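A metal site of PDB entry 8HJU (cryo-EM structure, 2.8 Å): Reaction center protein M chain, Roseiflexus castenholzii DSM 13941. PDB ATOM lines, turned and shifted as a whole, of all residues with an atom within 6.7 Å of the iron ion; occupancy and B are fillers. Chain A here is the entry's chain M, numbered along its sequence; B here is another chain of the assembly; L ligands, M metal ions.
ND1 of His 208 sits at hydrogen-bond distance from O2 of the ligand (2.6 Å).
The backbone carbonyl oxygen (O) of Ser 251 sits at hydrogen-bond distance from a ring nitrogen (ND1) of His 255, 2.9 Å away. ND1 of His 264 of chain B is in hydrogen-bond range of O of Glu 260 of chain B (2.6 Å).
Within 4 Å of the iron ion: His 208, Glu 223, His 255, His 229 of chain B and His 264 of chain B. The nearest printed residue that does not touch the iron ion is Val 233 of chain B (4.2 Å).
The iron ion is bound by OE2 of Glu 223 (1.8 Å), NE2 of His 229 of chain B (2.1 Å), NE2 of His 208 (2.2 Å), NE2 of His 255 (2.2 Å) and NE2 of His 264 of chain B (2.4 Å).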
ATOM      1  N   HIS A 208      19.960  12.786  25.474  1.00  0.00           N
ATOM      2  CA  HIS A 208      20.777  13.587  24.565  1.00  0.00           C
ATOM      3  C   HIS A 208      21.738  14.489  25.325  1.00  0.00           C
ATOM      4  O   HIS A 208      22.933  14.497  25.045  1.00  0.00           O
ATOM      5  CB  HIS A 208      19.889  14.405  23.627  1.00  0.00           C
ATOM      6  CG  HIS A 208      20.654  15.190  22.611  1.00  0.00           C
ATOM      7  ND1 HIS A 208      21.403  14.608  21.616  1.00  0.00           N
ATOM      8  CD2 HIS A 208      20.762  16.528  22.410  1.00  0.00           C
ATOM      9  CE1 HIS A 208      21.950  15.539  20.860  1.00  0.00           C
ATOM     10  NE2 HIS A 208      21.576  16.721  21.328  1.00  0.00           N
ATOM     11  N   ILE A 212      25.872  14.042  25.326  1.00  0.00           N
ATOM     12  CA  ILE A 212      26.748  15.077  24.790  1.00  0.00           C
ATOM     13  C   ILE A 212      27.656  15.628  25.887  1.00  0.00           C
ATOM     14  O   ILE A 212      28.800  15.992  25.629  1.00  0.00           O
ATOM     15  CB  ILE A 212      25.918  16.163  24.103  1.00  0.00           C
ATOM     16  CG1 ILE A 212      25.218  15.591  22.882  1.00  0.00           C
ATOM     17  CG2 ILE A 212      26.793  17.300  23.675  1.00  0.00           C
ATOM     18  CD1 ILE A 212      26.121  14.834  21.973  1.00  0.00           C
ATOM     19  N   SER A 220      31.772  16.956  21.249  1.00  0.00           N
ATOM     20  CA  SER A 220      30.559  16.437  20.636  1.00  0.00           C
ATOM     21  C   SER A 220      29.463  17.488  20.572  1.00  0.00           C
ATOM     22  O   SER A 220      28.529  17.338  19.771  1.00  0.00           O
ATOM     23  CB  SER A 220      30.062  15.230  21.408  1.00  0.00           C
ATOM     24  OG  SER A 220      29.554  15.614  22.672  1.00  0.00           O
ATOM     25  N   GLU A 221      29.542  18.532  21.396  1.00  0.00           N
ATOM     26  CA  GLU A 221      28.465  19.505  21.488  1.00  0.00           C
ATOM     27  C   GLU A 221      28.394  20.392  20.260  1.00  0.00           C
ATOM     28  O   GLU A 221      27.339  20.978  19.985  1.00  0.00           O
ATOM     29  CB  GLU A 221      28.627  20.352  22.743  1.00  0.00           C
ATOM     30  CG  GLU A 221      29.872  21.221  22.744  1.00  0.00           C
ATOM     31  CD  GLU A 221      31.069  20.522  23.354  1.00  0.00           C
ATOM     32  OE1 GLU A 221      31.887  21.198  24.002  1.00  0.00           O
ATOM     33  OE2 GLU A 221      31.181  19.293  23.196  1.00  0.00           O
ATOM     34  N   GLU A 223      27.504  20.572  17.275  1.00  0.00           N
ATOM     35  CA  GLU A 223      26.724  19.772  16.333  1.00  0.00           C
ATOM     36  C   GLU A 223      26.901  20.255  14.908  1.00  0.00           C
ATOM     37  O   GLU A 223      26.882  19.458  13.973  1.00  0.00           O
ATOM     38  CB  GLU A 223      25.252  19.794  16.719  1.00  0.00           C
ATOM     39  CG  GLU A 223      24.986  19.695  18.201  1.00  0.00           C
ATOM     40  CD  GLU A 223      24.703  18.291  18.633  1.00  0.00           C
ATOM     41  OE1 GLU A 223      25.071  17.362  17.904  1.00  0.00           O
ATOM     42  OE2 GLU A 223      24.080  18.116  19.699  1.00  0.00           O
ATOM     43  N   SER A 251      24.798  12.560  14.513  1.00  0.00           N
ATOM     44  CA  SER A 251      24.677  13.944  14.947  1.00  0.00           C
ATOM     45  C   SER A 251      23.423  14.608  14.401  1.00  0.00           C
ATOM     46  O   SER A 251      22.986  15.634  14.927  1.00  0.00           O
ATOM     47  CB  SER A 251      25.910  14.721  14.505  1.00  0.00           C
ATOM     48  OG  SER A 251      26.897  14.711  15.510  1.00  0.00           O
ATOM     49  N   ILE A 254      19.275  12.546  15.660  1.00  0.00           N
ATOM     50  CA  ILE A 254      18.786  12.665  17.025  1.00  0.00           C
ATOM     51  C   ILE A 254      17.967  13.934  17.192  1.00  0.00           C
ATOM     52  O   ILE A 254      16.999  13.962  17.954  1.00  0.00           O
ATOM     53  CB  ILE A 254      19.977  12.594  18.008  1.00  0.00           C
ATOM     54  CG1 ILE A 254      19.465  12.489  19.438  1.00  0.00           C
ATOM     55  CG2 ILE A 254      20.931  13.760  17.820  1.00  0.00           C
ATOM     56  CD1 ILE A 254      18.662  11.255  19.667  1.00  0.00           C
ATOM     57  N   HIS A 255      18.292  14.971  16.423  1.00  0.00           N
ATOM     58  CA  HIS A 255      17.533  16.203  16.528  1.00  0.00           C
ATOM     59  C   HIS A 255      16.224  16.136  15.767  1.00  0.00           C
ATOM     60  O   HIS A 255      15.247  16.780  16.155  1.00  0.00           O
ATOM     61  CB  HIS A 255      18.407  17.361  16.069  1.00  0.00           C
ATOM     62  CG  HIS A 255      19.692  17.459  16.826  1.00  0.00           C
ATOM     63  ND1 HIS A 255      20.867  16.896  16.380  1.00  0.00           N
ATOM     64  CD2 HIS A 255      19.973  17.998  18.035  1.00  0.00           C
ATOM     65  CE1 HIS A 255      21.819  17.110  17.262  1.00  0.00           C
ATOM     66  NE2 HIS A 255      21.308  17.775  18.274  1.00  0.00           N
ATOM     67  N   HIS B 229      15.862  22.866  20.941  1.00  0.00           N
ATOM     68  CA  HIS B 229      17.162  22.366  20.529  1.00  0.00           C
ATOM     69  C   HIS B 229      17.088  21.592  19.223  1.00  0.00           C
ATOM     70  O   HIS B 229      17.944  21.769  18.349  1.00  0.00           O
ATOM     71  CB  HIS B 229      17.762  21.488  21.633  1.00  0.00           C
ATOM     72  CG  HIS B 229      19.096  20.906  21.268  1.00  0.00           C
ATOM     73  ND1 HIS B 229      20.183  21.689  20.959  1.00  0.00           N
ATOM     74  CD2 HIS B 229      19.509  19.626  21.171  1.00  0.00           C
ATOM     75  CE1 HIS B 229      21.215  20.912  20.683  1.00  0.00           C
ATOM     76  NE2 HIS B 229      20.826  19.652  20.805  1.00  0.00           N
ATOM     77  N   VAL B 233      19.183  22.884  15.910  1.00  0.00           N
ATOM     78  CA  VAL B 233      20.156  22.079  15.183  1.00  0.00           C
ATOM     79  C   VAL B 233      19.643  21.730  13.797  1.00  0.00           C
ATOM     80  O   VAL B 233      20.411  21.674  12.828  1.00  0.00           O
ATOM     81  CB  VAL B 233      20.531  20.825  15.998  1.00  0.00           C
ATOM     82  CG1 VAL B 233      21.485  19.957  15.200  1.00  0.00           C
ATOM     83  CG2 VAL B 233      21.158  21.236  17.296  1.00  0.00           C
ATOM     84  N   GLU B 260      26.547  25.826  22.612  1.00  0.00           N
ATOM     85  CA  GLU B 260      26.430  24.409  22.269  1.00  0.00           C
ATOM     86  C   GLU B 260      26.539  23.538  23.502  1.00  0.00           C
ATOM     87  O   GLU B 260      25.730  22.625  23.700  1.00  0.00           O
ATOM     88  CB  GLU B 260      27.497  24.044  21.248  1.00  0.00           C
ATOM     89  CG  GLU B 260      27.320  24.708  19.903  1.00  0.00           C
ATOM     90  CD  GLU B 260      27.976  26.077  19.822  1.00  0.00           C
ATOM     91  OE1 GLU B 260      28.573  26.502  20.823  1.00  0.00           O
ATOM     92  OE2 GLU B 260      27.896  26.712  18.752  1.00  0.00           O
ATOM     93  N   ILE B 263      23.352  24.106  26.120  1.00  0.00           N
ATOM     94  CA  ILE B 263      22.021  23.573  25.896  1.00  0.00           C
ATOM     95  C   ILE B 263      21.974  22.088  26.260  1.00  0.00           C
ATOM     96  O   ILE B 263      20.945  21.599  26.729  1.00  0.00           O
ATOM     97  CB  ILE B 263      21.576  23.813  24.439  1.00  0.00           C
ATOM     98  CG1 ILE B 263      20.125  23.396  24.256  1.00  0.00           C
ATOM     99  CG2 ILE B 263      22.478  23.099  23.468  1.00  0.00           C
ATOM    100  CD1 ILE B 263      19.182  23.995  25.265  1.00  0.00           C
ATOM    101  N   HIS B 264      23.086  21.374  26.093  1.00  0.00           N
ATOM    102  CA  HIS B 264      23.092  19.967  26.452  1.00  0.00           C
ATOM    103  C   HIS B 264      23.206  19.770  27.956  1.00  0.00           C
ATOM    104  O   HIS B 264      22.580  18.867  28.520  1.00  0.00           O
ATOM    105  CB  HIS B 264      24.224  19.255  25.703  1.00  0.00           C
ATOM    106  CG  HIS B 264      24.074  19.301  24.219  1.00  0.00           C
ATOM    107  ND1 HIS B 264      24.619  20.302  23.440  1.00  0.00           N
ATOM    108  CD2 HIS B 264      23.416  18.479  23.364  1.00  0.00           C
ATOM    109  CE1 HIS B 264      24.313  20.079  22.177  1.00  0.00           C
ATOM    110  NE2 HIS B 264      23.582  18.987  22.108  1.00  0.00           N
HETATM  111  C1  LIG L   1      17.900  -5.828  24.649  1.00  0.00           C
HETATM  112  C2  LIG L   1      16.594  -1.185  24.675  1.00  0.00           C
HETATM  113  C3  LIG L   1      22.014  -7.532  26.605  1.00  0.00           C
HETATM  114  C4  LIG L   1      14.489   2.246  22.750  1.00  0.00           C
HETATM  115  C5  LIG L   1      13.073   6.416  21.264  1.00  0.00           C
HETATM  116  C6  LIG L   1      20.755 -12.082  26.277  1.00  0.00           C
HETATM  117  C7  LIG L   1      18.492  -6.160  25.997  1.00  0.00           C
HETATM  118  C8  LIG L   1      16.059  -2.537  25.053  1.00  0.00           C
HETATM  119  C9  LIG L   1      13.920   1.394  23.855  1.00  0.00           C
HETATM  120  C10 LIG L   1      21.887  -8.504  25.450  1.00  0.00           C
HETATM  121  C11 LIG L   1      13.029   5.723  22.622  1.00  0.00           C
HETATM  122  C12 LIG L   1      17.430   7.439  19.561  1.00  0.00           C
HETATM  123  C13 LIG L   1      20.012 -12.917  25.240  1.00  0.00           C
HETATM  124  C14 LIG L   1      16.836  -4.827  24.894  1.00  0.00           C
HETATM  125  C15 LIG L   1      15.484  -0.492  23.995  1.00  0.00           C
HETATM  126  C16 LIG L   1      20.664  -6.943  26.826  1.00  0.00           C
HETATM  127  C17 LIG L   1      16.265   8.195  20.174  1.00  0.00           C
HETATM  128  C18 LIG L   1      14.200   3.649  23.061  1.00  0.00           C
HETATM  129  C19 LIG L   1      16.513 -14.379  25.917  1.00  0.00           C
HETATM  130  C20 LIG L   1      20.807 -10.679  25.744  1.00  0.00           C
HETATM  131  C21 LIG L   1      14.274   7.275  21.259  1.00  0.00           C
HETATM  132  C22 LIG L   1      21.672   9.054  21.023  1.00  0.00           C
HETATM  133  C23 LIG L   1      20.770   7.911  21.267  1.00  0.00           C
HETATM  134  C24 LIG L   1      17.676 -13.667  25.297  1.00  0.00           C
HETATM  135  C25 LIG L   1      15.322 -13.431  25.814  1.00  0.00           C
HETATM  136  C26 LIG L   1      18.518   7.530  20.546  1.00  0.00           C
HETATM  137  C27 LIG L   1      17.116  -3.530  24.817  1.00  0.00           C
HETATM  138  C28 LIG L   1      19.834  -6.740  25.795  1.00  0.00           C
HETATM  139  C29 LIG L   1      15.031   0.657  24.485  1.00  0.00           C
HETATM  140  C30 LIG L   1      21.860  -9.889  25.975  1.00  0.00           C
HETATM  141  C31 LIG L   1      13.312   4.307  22.351  1.00  0.00           C
HETATM  142  C32 LIG L   1      15.068   7.314  20.180  1.00  0.00           C
HETATM  143  C33 LIG L   1      18.873 -13.631  25.893  1.00  0.00           C
HETATM  144  C34 LIG L   1      11.622 -14.352  26.185  1.00  0.00           C
HETATM  145  C35 LIG L   1      21.581  10.147  21.763  1.00  0.00           C
HETATM  146  C36 LIG L   1      19.761   7.844  20.201  1.00  0.00           C
HETATM  147  C37 LIG L   1      12.886 -13.641  25.830  1.00  0.00           C
HETATM  148  C38 LIG L   1      14.071 -14.157  26.161  1.00  0.00           C
HETATM  149  C39 LIG L   1      10.837 -13.404  27.093  1.00  0.00           C
HETATM  150  C40 LIG L   1      23.562  10.019  19.711  1.00  0.00           C
HETATM  151  C41 LIG L   1      22.664   8.890  19.945  1.00  0.00           C
HETATM  152  C42 LIG L   1      23.466  11.163  20.479  1.00  0.00           C
HETATM  153  C43 LIG L   1      22.464  11.293  21.547  1.00  0.00           C
HETATM  154  C44 LIG L   1      15.488  -5.327  25.211  1.00  0.00           C
HETATM  155  C45 LIG L   1      14.913  -1.151  22.803  1.00  0.00           C
HETATM  156  C46 LIG L   1      20.290  -6.617  28.220  1.00  0.00           C
HETATM  157  C47 LIG L   1      14.947   4.291  24.156  1.00  0.00           C
HETATM  158  C48 LIG L   1      19.639 -10.207  24.974  1.00  0.00           C
HETATM  159  C49 LIG L   1      14.523   8.054  22.446  1.00  0.00           C
HETATM  160  C50 LIG L   1      17.436 -13.009  23.984  1.00  0.00           C
HETATM  161  C51 LIG L   1      18.192   7.287  21.964  1.00  0.00           C
HETATM  162  C52 LIG L   1       9.625 -14.098  27.554  1.00  0.00           C
HETATM  163  C53 LIG L   1       8.413 -13.758  27.095  1.00  0.00           C
HETATM  164  C54 LIG L   1       7.228 -14.491  27.592  1.00  0.00           C
HETATM  165  C55 LIG L   1      20.562  10.265  22.839  1.00  0.00           C
HETATM  166  C56 LIG L   1      12.761 -12.347  25.117  1.00  0.00           C
HETATM  167  C57 LIG L   1      24.502   9.927  18.716  1.00  0.00           C
HETATM  168  C58 LIG L   1      24.312  12.214  20.242  1.00  0.00           C
HETATM  169  C59 LIG L   1       6.261 -14.700  26.446  1.00  0.00           C
HETATM  170  C60 LIG L   1      25.361  10.976  18.479  1.00  0.00           C
HETATM  171  C61 LIG L   1      25.267  12.119  19.238  1.00  0.00           C
HETATM  172  C62 LIG L   1       8.204 -12.664  26.125  1.00  0.00           C
HETATM  173  C63 LIG L   1       4.933 -14.764  27.074  1.00  0.00           C
HETATM  174  C64 LIG L   1       3.902 -14.070  26.616  1.00  0.00           C
HETATM  175  C65 LIG L   1       2.612 -14.193  27.342  1.00  0.00           C
HETATM  176  C66 LIG L   1       3.971 -13.156  25.436  1.00  0.00           C
HETATM  177  O1  LIG L   1      22.741   7.886  19.281  1.00  0.00           O
HETATM  178  O2  LIG L   1      22.381  12.305  22.210  1.00  0.00           O
HETATM  179 FE    FE M   1      22.331  18.381  20.182  1.00  0.00          FE
